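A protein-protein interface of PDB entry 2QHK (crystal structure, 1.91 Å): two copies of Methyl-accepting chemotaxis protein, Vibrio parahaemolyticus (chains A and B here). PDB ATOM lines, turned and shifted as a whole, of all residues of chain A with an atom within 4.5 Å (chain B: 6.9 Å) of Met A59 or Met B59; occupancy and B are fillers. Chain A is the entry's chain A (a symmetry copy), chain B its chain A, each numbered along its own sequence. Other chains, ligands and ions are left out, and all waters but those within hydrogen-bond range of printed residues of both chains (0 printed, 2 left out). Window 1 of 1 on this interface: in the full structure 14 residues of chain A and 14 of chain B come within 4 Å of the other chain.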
ATOM      1  N   MET A  31     -14.663 -17.837  -1.778  1.00  0.00           N
ATOM      2  CA  MET A  31     -13.867 -17.911  -3.006  1.00  0.00           C
ATOM      3  C   MET A  31     -12.871 -16.767  -3.138  1.00  0.00           C
ATOM      4  O   MET A  31     -11.722 -16.975  -3.556  1.00  0.00           O
ATOM      5  CB  MET A  31     -14.798 -18.009  -4.224  1.00  0.00           C
ATOM      6  CG  MET A  31     -15.583 -19.294  -4.220  1.00  0.00           C
ATOM      7  SD  MET A  31     -14.514 -20.736  -5.116  1.00  0.00           S
ATOM      8  CE  MET A  31     -15.092 -20.353  -6.984  1.00  0.00           C
ATOM      9  N   GLY A  32     -13.306 -15.563  -2.769  1.00  0.00           N
ATOM     10  CA  GLY A  32     -12.458 -14.400  -2.874  1.00  0.00           C
ATOM     11  C   GLY A  32     -11.358 -14.448  -1.816  1.00  0.00           C
ATOM     12  O   GLY A  32     -10.197 -14.232  -2.119  1.00  0.00           O
ATOM     13  N   THR A  34     -10.130 -17.107  -0.281  1.00  0.00           N
ATOM     14  CA  THR A  34      -9.208 -18.204  -0.549  1.00  0.00           C
ATOM     15  C   THR A  34      -8.348 -17.946  -1.795  1.00  0.00           C
ATOM     16  O   THR A  34      -7.189 -18.340  -1.816  1.00  0.00           O
ATOM     17  CB  THR A  34      -9.939 -19.590  -0.595  1.00  0.00           C
ATOM     18  OG1 THR A  34     -11.003 -19.552  -1.540  1.00  0.00           O
ATOM     19  CG2 THR A  34     -10.545 -19.902   0.804  1.00  0.00           C
ATOM     20  N   ALA A  35      -8.903 -17.276  -2.804  1.00  0.00           N
ATOM     21  CA  ALA A  35      -8.140 -16.901  -4.006  1.00  0.00           C
ATOM     22  C   ALA A  35      -6.901 -16.070  -3.679  1.00  0.00           C
ATOM     23  O   ALA A  35      -5.864 -16.199  -4.362  1.00  0.00           O
ATOM     24  CB  ALA A  35      -9.011 -16.166  -4.985  1.00  0.00           C
ATOM     25  N   ILE A  55      -6.449  -9.432  -8.466  1.00  0.00           N
ATOM     26  CA  ILE A  55      -7.227 -10.656  -8.523  1.00  0.00           C
ATOM     27  C   ILE A  55      -8.674 -10.350  -8.108  1.00  0.00           C
ATOM     28  O   ILE A  55      -9.616 -10.678  -8.839  1.00  0.00           O
ATOM     29  CB  ILE A  55      -6.629 -11.763  -7.607  1.00  0.00           C
ATOM     30  CG1 ILE A  55      -5.253 -12.216  -8.127  1.00  0.00           C
ATOM     31  CG2 ILE A  55      -7.581 -12.950  -7.514  1.00  0.00           C
ATOM     32  CD1 ILE A  55      -4.410 -12.924  -7.078  1.00  0.00           C
ATOM     33  N   LEU A  56      -8.855  -9.695  -6.965  1.00  0.00           N
ATOM     34  CA  LEU A  56     -10.234  -9.472  -6.481  1.00  0.00           C
ATOM     35  C   LEU A  56     -11.051  -8.576  -7.401  1.00  0.00           C
ATOM     36  O   LEU A  56     -12.247  -8.808  -7.595  1.00  0.00           O
ATOM     37  CB  LEU A  56     -10.240  -8.913  -5.061  1.00  0.00           C
ATOM     38  CG  LEU A  56      -9.782  -9.866  -3.942  1.00  0.00           C
ATOM     39  CD1 LEU A  56      -9.461  -9.049  -2.724  1.00  0.00           C
ATOM     40  CD2 LEU A  56     -10.842 -10.944  -3.631  1.00  0.00           C
ATOM     41  N   LYS A  57     -10.413  -7.561  -7.983  1.00  0.00           N
ATOM     42  CA  LYS A  57     -11.131  -6.679  -8.902  1.00  0.00           C
ATOM     43  C   LYS A  57     -11.526  -7.341 -10.232  1.00  0.00           C
ATOM     44  O   LYS A  57     -12.456  -6.884 -10.902  1.00  0.00           O
ATOM     45  CB  LYS A  57     -10.316  -5.409  -9.153  1.00  0.00           C
ATOM     46  CG  LYS A  57     -10.309  -4.481  -7.945  1.00  0.00           C
ATOM     47  CD  LYS A  57      -9.271  -3.344  -8.100  1.00  0.00           C
ATOM     48  CE  LYS A  57      -9.615  -2.362  -9.185  1.00  0.00           C
ATOM     49  NZ  LYS A  57      -8.506  -1.351  -9.283  1.00  0.00           N
ATOM     50  N   ALA A  58     -10.835  -8.408 -10.621  1.00  0.00           N
ATOM     51  CA  ALA A  58     -11.212  -9.135 -11.857  1.00  0.00           C
ATOM     52  C   ALA A  58     -12.381 -10.111 -11.661  1.00  0.00           C
ATOM     53  O   ALA A  58     -13.112 -10.426 -12.609  1.00  0.00           O
ATOM     54  CB  ALA A  58     -10.005  -9.878 -12.406  1.00  0.00           C
ATOM     55  N   MET A  59     -12.529 -10.630 -10.441  1.00  0.00           N
ATOM     56  CA  MET A  59     -13.524 -11.671 -10.165  1.00  0.00           C
ATOM     57  C   MET A  59     -14.991 -11.275 -10.345  1.00  0.00           C
ATOM     58  O   MET A  59     -15.425 -10.196  -9.921  1.00  0.00           O
ATOM     59  CB  MET A  59     -13.292 -12.258  -8.760  1.00  0.00           C
ATOM     60  CG  MET A  59     -12.042 -13.091  -8.709  1.00  0.00           C
ATOM     61  SD  MET A  59     -11.561 -13.627  -6.883  1.00  0.00           S
ATOM     62  CE  MET A  59     -12.828 -15.044  -6.710  1.00  0.00           C
ATOM     63  N   ARG A  60     -15.759 -12.161 -10.972  1.00  0.00           N
ATOM     64  CA  ARG A  60     -17.223 -11.975 -11.060  1.00  0.00           C
ATOM     65  C   ARG A  60     -17.935 -13.304 -10.796  1.00  0.00           C
ATOM     66  O   ARG A  60     -17.434 -14.351 -11.205  1.00  0.00           O
ATOM     67  CB  ARG A  60     -17.622 -11.474 -12.462  1.00  0.00           C
ATOM     68  CG  ARG A  60     -17.016 -10.162 -12.870  1.00  0.00           C
ATOM     69  CD  ARG A  60     -17.660  -8.991 -12.108  1.00  0.00           C
ATOM     70  NE  ARG A  60     -17.203  -7.707 -12.656  1.00  0.00           N
ATOM     71  CZ  ARG A  60     -16.007  -7.172 -12.411  1.00  0.00           C
ATOM     72  NH1 ARG A  60     -15.140  -7.790 -11.595  1.00  0.00           N
ATOM     73  NH2 ARG A  60     -15.689  -5.990 -12.948  1.00  0.00           N
ATOM     74  N   GLY A  65     -22.058  -9.120  -9.938  1.00  0.00           N
ATOM     75  CA  GLY A  65     -21.499  -9.837  -8.778  1.00  0.00           C
ATOM     76  C   GLY A  65     -20.008  -9.602  -8.672  1.00  0.00           C
ATOM     77  O   GLY A  65     -19.223 -10.262  -9.372  1.00  0.00           O
ATOM     78  N   TYR A  66     -19.604  -8.674  -7.791  1.00  0.00           N
ATOM     79  CA  TYR A  66     -18.232  -8.190  -7.750  1.00  0.00           C
ATOM     80  C   TYR A  66     -17.820  -7.844  -6.320  1.00  0.00           C
ATOM     81  O   TYR A  66     -18.682  -7.760  -5.423  1.00  0.00           O
ATOM     82  CB  TYR A  66     -18.101  -6.916  -8.636  1.00  0.00           C
ATOM     83  CG  TYR A  66     -18.946  -5.750  -8.106  1.00  0.00           C
ATOM     84  CD1 TYR A  66     -18.428  -4.868  -7.162  1.00  0.00           C
ATOM     85  CD2 TYR A  66     -20.273  -5.571  -8.524  1.00  0.00           C
ATOM     86  CE1 TYR A  66     -19.185  -3.793  -6.656  1.00  0.00           C
ATOM     87  CE2 TYR A  66     -21.068  -4.497  -8.021  1.00  0.00           C
ATOM     88  CZ  TYR A  66     -20.506  -3.619  -7.090  1.00  0.00           C
ATOM     89  OH  TYR A  66     -21.252  -2.577  -6.596  1.00  0.00           O
ATOM     90  N   PHE A  67     -16.510  -7.619  -6.124  1.00  0.00           N
ATOM     91  CA  PHE A  67     -15.952  -7.238  -4.823  1.00  0.00           C
ATOM     92  C   PHE A  67     -15.614  -5.751  -4.664  1.00  0.00           C
ATOM     93  O   PHE A  67     -15.223  -5.072  -5.635  1.00  0.00           O
ATOM     94  CB  PHE A  67     -14.664  -8.022  -4.549  1.00  0.00           C
ATOM     95  CG  PHE A  67     -14.887  -9.454  -4.295  1.00  0.00           C
ATOM     96  CD1 PHE A  67     -15.337  -9.890  -3.046  1.00  0.00           C
ATOM     97  CD2 PHE A  67     -14.633 -10.398  -5.291  1.00  0.00           C
ATOM     98  CE1 PHE A  67     -15.546 -11.252  -2.789  1.00  0.00           C
ATOM     99  CE2 PHE A  67     -14.823 -11.761  -5.055  1.00  0.00           C
ATOM    100  CZ  PHE A  67     -15.289 -12.203  -3.806  1.00  0.00           C
ATOM    101  N   TYR B  28     -19.591 -20.422  -9.672  1.00  0.00           N
ATOM    102  CA  TYR B  28     -18.282 -20.805  -9.175  1.00  0.00           C
ATOM    103  C   TYR B  28     -17.269 -20.876 -10.303  1.00  0.00           C
ATOM    104  O   TYR B  28     -16.149 -20.395 -10.141  1.00  0.00           O
ATOM    105  CB  TYR B  28     -18.349 -22.175  -8.466  1.00  0.00           C
ATOM    106  CG  TYR B  28     -19.317 -22.203  -7.280  1.00  0.00           C
ATOM    107  CD1 TYR B  28     -19.493 -21.078  -6.483  1.00  0.00           C
ATOM    108  CD2 TYR B  28     -19.995 -23.375  -6.943  1.00  0.00           C
ATOM    109  CE1 TYR B  28     -20.366 -21.098  -5.391  1.00  0.00           C
ATOM    110  CE2 TYR B  28     -20.864 -23.418  -5.859  1.00  0.00           C
ATOM    111  CZ  TYR B  28     -21.032 -22.290  -5.081  1.00  0.00           C
ATOM    112  OH  TYR B  28     -21.899 -22.326  -4.010  1.00  0.00           O
ATOM    113  N   MET B  30     -17.322 -19.294 -13.160  1.00  0.00           N
ATOM    114  CA  MET B  30     -17.066 -17.904 -13.544  1.00  0.00           C
ATOM    115  C   MET B  30     -16.058 -17.225 -12.624  1.00  0.00           C
ATOM    116  O   MET B  30     -15.169 -16.528 -13.083  1.00  0.00           O
ATOM    117  CB  MET B  30     -18.337 -17.064 -13.592  1.00  0.00           C
ATOM    118  CG  MET B  30     -18.065 -15.699 -14.191  1.00  0.00           C
ATOM    119  SD  MET B  30     -19.688 -14.645 -14.353  1.00  0.00           S
ATOM    120  CE  MET B  30     -20.598 -15.472 -15.895  1.00  0.00           C
ATOM    121  N   MET B  31     -16.183 -17.466 -11.324  1.00  0.00           N
ATOM    122  CA  MET B  31     -15.247 -16.895 -10.353  1.00  0.00           C
ATOM    123  C   MET B  31     -13.809 -17.342 -10.581  1.00  0.00           C
ATOM    124  O   MET B  31     -12.873 -16.535 -10.474  1.00  0.00           O
ATOM    125  CB  MET B  31     -15.726 -17.201  -8.926  1.00  0.00           C
ATOM    126  CG  MET B  31     -17.032 -16.516  -8.621  1.00  0.00           C
ATOM    127  SD  MET B  31     -16.673 -14.664  -7.936  1.00  0.00           S
ATOM    128  CE  MET B  31     -16.441 -15.147  -6.016  1.00  0.00           C
ATOM    129  N   GLY B  32     -13.636 -18.621 -10.911  1.00  0.00           N
ATOM    130  CA  GLY B  32     -12.315 -19.162 -11.127  1.00  0.00           C
ATOM    131  C   GLY B  32     -11.732 -18.631 -12.436  1.00  0.00           C
ATOM    132  O   GLY B  32     -10.597 -18.189 -12.472  1.00  0.00           O
ATOM    133  N   VAL B  33     -12.543 -18.638 -13.492  1.00  0.00           N
ATOM    134  CA  VAL B  33     -12.110 -18.126 -14.795  1.00  0.00           C
ATOM    135  C   VAL B  33     -11.739 -16.623 -14.758  1.00  0.00           C
ATOM    136  O   VAL B  33     -10.746 -16.186 -15.373  1.00  0.00           O
ATOM    137  CB  VAL B  33     -13.166 -18.425 -15.893  1.00  0.00           C
ATOM    138  CG1 VAL B  33     -12.809 -17.698 -17.238  1.00  0.00           C
ATOM    139  CG2 VAL B  33     -13.257 -19.936 -16.111  1.00  0.00           C
ATOM    140  N   THR B  34     -12.528 -15.848 -14.035  1.00  0.00           N
ATOM    141  CA  THR B  34     -12.278 -14.415 -13.939  1.00  0.00           C
ATOM    142  C   THR B  34     -11.111 -14.092 -12.995  1.00  0.00           C
ATOM    143  O   THR B  34     -10.371 -13.153 -13.255  1.00  0.00           O
ATOM    144  CB  THR B  34     -13.578 -13.612 -13.594  1.00  0.00           C
ATOM    145  OG1 THR B  34     -14.169 -14.124 -12.403  1.00  0.00           O
ATOM    146  CG2 THR B  34     -14.607 -13.769 -14.750  1.00  0.00           C
ATOM    147  N   ALA B  35     -10.943 -14.873 -11.927  1.00  0.00           N
ATOM    148  CA  ALA B  35      -9.807 -14.704 -11.007  1.00  0.00           C
ATOM    149  C   ALA B  35      -8.457 -14.793 -11.718  1.00  0.00           C
ATOM    150  O   ALA B  35      -7.500 -14.092 -11.329  1.00  0.00           O
ATOM    151  CB  ALA B  35      -9.869 -15.706  -9.890  1.00  0.00           C
ATOM    152  N   ILE B  36      -8.368 -15.674 -12.725  1.00  0.00           N
ATOM    153  CA  ILE B  36      -7.113 -15.848 -13.472  1.00  0.00           C
ATOM    154  C   ILE B  36      -7.111 -15.070 -14.789  1.00  0.00           C
ATOM    155  O   ILE B  36      -6.143 -15.120 -15.547  1.00  0.00           O
ATOM    156  CB  ILE B  36      -6.790 -17.352 -13.730  1.00  0.00           C
ATOM    157  CG1 ILE B  36      -7.871 -17.985 -14.639  1.00  0.00           C
ATOM    158  CG2 ILE B  36      -6.642 -18.096 -12.397  1.00  0.00           C
ATOM    159  CD1 ILE B  36      -7.402 -19.160 -15.508  1.00  0.00           C
ATOM    160  N   PRO B  38      -6.621 -11.853 -15.649  1.00  0.00           N
ATOM    161  CA  PRO B  38      -5.470 -10.962 -15.926  1.00  0.00           C
ATOM    162  C   PRO B  38      -4.241 -11.761 -16.380  1.00  0.00           C
ATOM    163  O   PRO B  38      -3.600 -11.399 -17.369  1.00  0.00           O
ATOM    164  CB  PRO B  38      -5.203 -10.309 -14.570  1.00  0.00           C
ATOM    165  CG  PRO B  38      -6.537 -10.343 -13.877  1.00  0.00           C
ATOM    166  CD  PRO B  38      -7.135 -11.661 -14.279  1.00  0.00           C
ATOM    167  N   GLU B  54      -1.551 -21.627  -8.931  1.00  0.00           N
ATOM    168  CA  GLU B  54      -1.473 -21.341  -7.498  1.00  0.00           C
ATOM    169  C   GLU B  54      -2.720 -20.667  -6.930  1.00  0.00           C
ATOM    170  O   GLU B  54      -3.108 -20.913  -5.770  1.00  0.00           O
ATOM    171  CB  GLU B  54      -0.200 -20.548  -7.201  1.00  0.00           C
ATOM    172  CG  GLU B  54       1.045 -21.402  -7.404  1.00  0.00           C
ATOM    173  CD  GLU B  54       2.338 -20.644  -7.252  1.00  0.00           C
ATOM    174  OE1 GLU B  54       2.332 -19.543  -6.656  1.00  0.00           O
ATOM    175  OE2 GLU B  54       3.370 -21.165  -7.725  1.00  0.00           O
ATOM    176  N   ILE B  55      -3.360 -19.840  -7.753  1.00  0.00           N
ATOM    177  CA  ILE B  55      -4.611 -19.198  -7.395  1.00  0.00           C
ATOM    178  C   ILE B  55      -5.738 -20.241  -7.429  1.00  0.00           C
ATOM    179  O   ILE B  55      -6.476 -20.396  -6.448  1.00  0.00           O
ATOM    180  CB  ILE B  55      -4.947 -18.015  -8.351  1.00  0.00           C
ATOM    181  CG1 ILE B  55      -3.926 -16.876  -8.185  1.00  0.00           C
ATOM    182  CG2 ILE B  55      -6.360 -17.507  -8.094  1.00  0.00           C
ATOM    183  CD1 ILE B  55      -3.891 -15.916  -9.364  1.00  0.00           C
ATOM    184  N   LEU B  56      -5.851 -20.982  -8.528  1.00  0.00           N
ATOM    185  CA  LEU B  56      -6.984 -21.924  -8.640  1.00  0.00           C
ATOM    186  C   LEU B  56      -6.935 -23.041  -7.606  1.00  0.00           C
ATOM    187  O   LEU B  56      -7.974 -23.448  -7.082  1.00  0.00           O
ATOM    188  CB  LEU B  56      -7.079 -22.512 -10.045  1.00  0.00           C
ATOM    189  CG  LEU B  56      -7.503 -21.549 -11.169  1.00  0.00           C
ATOM    190  CD1 LEU B  56      -7.145 -22.171 -12.488  1.00  0.00           C
ATOM    191  CD2 LEU B  56      -9.007 -21.206 -11.100  1.00  0.00           C
ATOM    192  N   LYS B  57      -5.734 -23.528  -7.296  1.00  0.00           N
ATOM    193  CA  LYS B  57      -5.612 -24.580  -6.290  1.00  0.00           C
ATOM    194  C   LYS B  57      -5.920 -24.120  -4.856  1.00  0.00           C
ATOM    195  O   LYS B  57      -6.257 -24.940  -3.998  1.00  0.00           O
ATOM    196  CB  LYS B  57      -4.224 -25.219  -6.366  1.00  0.00           C
ATOM    197  CG  LYS B  57      -4.060 -26.099  -7.598  1.00  0.00           C
ATOM    198  CD  LYS B  57      -2.586 -26.515  -7.815  1.00  0.00           C
ATOM    199  CE  LYS B  57      -2.064 -27.447  -6.756  1.00  0.00           C
ATOM    200  NZ  LYS B  57      -0.613 -27.724  -7.038  1.00  0.00           N
ATOM    201  N   ALA B  58      -5.808 -22.823  -4.585  1.00  0.00           N
ATOM    202  CA  ALA B  58      -6.160 -22.305  -3.242  1.00  0.00           C
ATOM    203  C   ALA B  58      -7.669 -22.096  -3.042  1.00  0.00           C
ATOM    204  O   ALA B  58      -8.170 -22.135  -1.909  1.00  0.00           O
ATOM    205  CB  ALA B  58      -5.419 -21.003  -2.981  1.00  0.00           C
ATOM    206  N   MET B  59      -8.385 -21.826  -4.132  1.00  0.00           N
ATOM    207  CA  MET B  59      -9.807 -21.477  -4.051  1.00  0.00           C
ATOM    208  C   MET B  59     -10.744 -22.562  -3.515  1.00  0.00           C
ATOM    209  O   MET B  59     -10.649 -23.739  -3.888  1.00  0.00           O
ATOM    210  CB  MET B  59     -10.301 -20.965  -5.417  1.00  0.00           C
ATOM    211  CG  MET B  59      -9.733 -19.612  -5.736  1.00  0.00           C
ATOM    212  SD  MET B  59     -10.111 -19.045  -7.578  1.00  0.00           S
ATOM    213  CE  MET B  59     -11.921 -18.511  -7.295  1.00  0.00           C
ATOM    214  N   ARG B  60     -11.659 -22.159  -2.638  1.00  0.00           N
ATOM    215  CA  ARG B  60     -12.726 -23.070  -2.175  1.00  0.00           C
ATOM    216  C   ARG B  60     -14.065 -22.330  -2.136  1.00  0.00           C
ATOM    217  O   ARG B  60     -14.092 -21.146  -1.797  1.00  0.00           O
ATOM    218  CB  ARG B  60     -12.414 -23.596  -0.761  1.00  0.00           C
ATOM    219  CG  ARG B  60     -11.131 -24.367  -0.632  1.00  0.00           C
ATOM    220  CD  ARG B  60     -11.250 -25.757  -1.281  1.00  0.00           C
ATOM    221  NE  ARG B  60     -10.065 -26.570  -0.976  1.00  0.00           N
ATOM    222  CZ  ARG B  60      -8.883 -26.423  -1.575  1.00  0.00           C
ATOM    223  NH1 ARG B  60      -8.719 -25.510  -2.542  1.00  0.00           N
ATOM    224  NH2 ARG B  60      -7.867 -27.222  -1.235  1.00  0.00           N
ATOM    225  N   PHE B  61     -15.168 -23.017  -2.461  1.00  0.00           N
ATOM    226  CA  PHE B  61     -16.488 -22.502  -2.071  1.00  0.00           C
ATOM    227  C   PHE B  61     -17.125 -23.254  -0.897  1.00  0.00           C
ATOM    228  O   PHE B  61     -18.198 -22.863  -0.406  1.00  0.00           O
ATOM    229  CB  PHE B  61     -17.452 -22.415  -3.270  1.00  0.00           C
ATOM    230  CG  PHE B  61     -17.641 -23.722  -4.029  1.00  0.00           C
ATOM    231  CD1 PHE B  61     -18.652 -24.607  -3.684  1.00  0.00           C
ATOM    232  CD2 PHE B  61     -16.830 -24.038  -5.102  1.00  0.00           C
ATOM    233  CE1 PHE B  61     -18.842 -25.813  -4.414  1.00  0.00           C
ATOM    234  CE2 PHE B  61     -17.015 -25.241  -5.838  1.00  0.00           C
ATOM    235  CZ  PHE B  61     -18.022 -26.120  -5.475  1.00  0.00           C
ATOM    236  N   GLU B  62     -16.466 -24.341  -0.488  1.00  0.00           N
ATOM    237  CA  GLU B  62     -16.766 -25.094   0.735  1.00  0.00           C
ATOM    238  C   GLU B  62     -15.641 -26.122   0.825  1.00  0.00           C
ATOM    239  O   GLU B  62     -14.813 -26.221  -0.078  1.00  0.00           O
ATOM    240  CB  GLU B  62     -18.144 -25.778   0.666  1.00  0.00           C
ATOM    241  CG  GLU B  62     -18.328 -26.680  -0.574  1.00  0.00           C
ATOM    242  CD  GLU B  62     -19.729 -27.328  -0.670  1.00  0.00           C
ATOM    243  OE1 GLU B  62     -20.575 -27.098   0.201  1.00  0.00           O
ATOM    244  OE2 GLU B  62     -19.984 -28.082  -1.628  1.00  0.00           O
ATOM    245  N   GLY B  65     -15.468 -28.097  -2.175  1.00  0.00           N
ATOM    246  CA  GLY B  65     -15.698 -27.287  -3.384  1.00  0.00           C
ATOM    247  C   GLY B  65     -14.394 -26.720  -3.904  1.00  0.00           C
ATOM    248  O   GLY B  65     -13.912 -25.697  -3.391  1.00  0.00           O
ATOM    249  N   TYR B  66     -13.822 -27.368  -4.930  1.00  0.00           N
ATOM    250  CA  TYR B  66     -12.467 -27.071  -5.373  1.00  0.00           C
ATOM    251  C   TYR B  66     -12.337 -27.261  -6.885  1.00  0.00           C
ATOM    252  O   TYR B  66     -13.234 -27.849  -7.520  1.00  0.00           O
ATOM    253  CB  TYR B  66     -11.462 -28.019  -4.656  1.00  0.00           C
ATOM    254  CG  TYR B  66     -11.685 -29.491  -5.029  1.00  0.00           C
ATOM    255  CD1 TYR B  66     -11.059 -30.045  -6.142  1.00  0.00           C
ATOM    256  CD2 TYR B  66     -12.556 -30.300  -4.284  1.00  0.00           C
ATOM    257  CE1 TYR B  66     -11.251 -31.392  -6.506  1.00  0.00           C
ATOM    258  CE2 TYR B  66     -12.778 -31.666  -4.637  1.00  0.00           C
ATOM    259  CZ  TYR B  66     -12.116 -32.193  -5.749  1.00  0.00           C
ATOM    260  OH  TYR B  66     -12.313 -33.505  -6.104  1.00  0.00           O
ATOM    261  N   PHE B  67     -11.210 -26.788  -7.442  1.00  0.00           N
ATOM    262  CA  PHE B  67     -10.909 -26.923  -8.869  1.00  0.00           C
ATOM    263  C   PHE B  67      -9.905 -28.025  -9.228  1.00  0.00           C
ATOM    264  O   PHE B  67      -8.975 -28.324  -8.453  1.00  0.00           O
ATOM    265  CB  PHE B  67     -10.344 -25.608  -9.418  1.00  0.00           C
ATOM    266  CG  PHE B  67     -11.337 -24.523  -9.492  1.00  0.00           C
ATOM    267  CD1 PHE B  67     -12.264 -24.482 -10.537  1.00  0.00           C
ATOM    268  CD2 PHE B  67     -11.353 -23.512  -8.531  1.00  0.00           C
ATOM    269  CE1 PHE B  67     -13.209 -23.452 -10.623  1.00  0.00           C
ATOM    270  CE2 PHE B  67     -12.279 -22.468  -8.602  1.00  0.00           C
ATOM    271  CZ  PHE B  67     -13.222 -22.430  -9.643  1.00  0.00           C
ATOM    272  N   ALA B  80      -6.447 -29.396  -6.884  1.00  0.00           N
ATOM    273  CA  ALA B  80      -6.382 -28.665  -5.612  1.00  0.00           C
ATOM    274  C   ALA B  80      -6.228 -29.604  -4.411  1.00  0.00           C
ATOM    275  O   ALA B  80      -5.602 -29.241  -3.416  1.00  0.00           O
ATOM    276  CB  ALA B  80      -7.634 -27.793  -5.418  1.00  0.00           C
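Hydrophobic or aromatic side chains of chain A that line the printed part of chain B: Met A31, Ala A35, Ile A55, Ala A58, Met A59 and Phe A67.
Among the printed residues, 23 pairs touch across the chains.
Among the printed residues, no Asp or Glu carboxylate lies within 4 Å of a Lys or Arg side-chain nitrogen of the other chain.
Among the printed residues, merely in contact across the chains: Met A31 with Tyr B28, Arg A60 with Met B30, Thr A34 with Ala B58, Ala A58 with Thr B34, Thr A34 with Met B59, Met A59 with Thr B34, Met A59 with Ala B35, Ala A35 with Met B59, Met A59 with Met B59, Met A31 with Met B59, Met A59 with Met B31, Met A31 with Met B31, Ala A58 with Pro B38, Ile A55 with Ile B55, Phe A67 with Met B31, Met A31 with Phe B67, Ile A55 with Ala B35 and Ala A35 with Ile B55.
Met A31 touches Arg B60, and with the chains exchanged Arg A60 touches Met B31.
Thr A34 touches Met B59, and with the chains exchanged Met A59 touches Thr B34.
Thr A34 touches Arg B60, and with the chains exchanged Arg A60 touches Thr B34.
Met B59 touches its own counterpart, Met A59.
Of the 23 pairs that touch across the chains among the printed residues, 19 have their exchanged pair printed and touching as well.
Printed residues of chain B within 4 Å of Ala A35: Ile B55 and Met B59.
Of the printed residues of chain B, Ile A55 touches Ala B35 (3.98 Å) and Ile B55 (3.8 Å).
Met A59 touches four residues of chain B.
Of the printed residues of chain A, Met B30 touches Arg A60 (3.3 Å).
Of the printed residues of chain A, Pro B38 touches Ala A58 (3.8 Å).
Printed residues of chain A within 4 Å of Ala B58: Thr A34.
Of chain A, only Met A31, Thr A34, Ala A35 and Met A59 come within 4 Å of Met B59.
The nearest residue of chain B that does not touch Met A59 is Gly B32 (5.6 Å).
The nearest printed residue of chain A that does not touch Met B59 is Gly A32 (5.6 Å).
The nearest printed residue of chain B that does not touch Met A31 is Gly B32 (4.5 Å).
The backbone carbonyl oxygen (O) of Arg A60 is in hydrogen-bond range of the backbone NH (N) of Met B31, 3.4 Å away.
N of Arg A60 sits at hydrogen-bond distance from OG1 of Thr B34 (2.9 Å).
The backbone carbonyl oxygen (O) of Arg B60 lies within hydrogen-bond range of the backbone NH (N) of Met A31, 3.4 Å away.
The side-chain hydroxyl of Thr A34 lies within hydrogen-bond range of the backbone NH of Arg B60 (2.9 Å).
The backbone NH (N) of Phe B61 is in hydrogen-bond range of the side-chain sulfur (SD) of Met A31 (3.6 Å).
O of Met B30 lies within hydrogen-bond range of OG1 of Thr B34 (2.7 Å).
The backbone carbonyl oxygen of Met B31 is in hydrogen-bond range of the side-chain hydroxyl of Thr B34 (3.3 Å).
The guanidinium group (NH1) of Arg B60 sits at hydrogen-bond distance from the backbone carbonyl oxygen (O) of Ala B58 (3.5 Å).
The backbone carbonyl oxygen (O) of Phe B67 sits at hydrogen-bond distance from the backbone NH (N) of Ala B80, at 3.2 Å.
The guanidinium group (NH1) of Arg A60 is in hydrogen-bond range of the backbone carbonyl oxygen (O) of Lys A57 (2.9 Å).
The backbone carbonyl oxygen (O) of Ala A58 lies within hydrogen-bond range of the guanidinium group (NH1) of Arg A60, 3.5 Å away.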
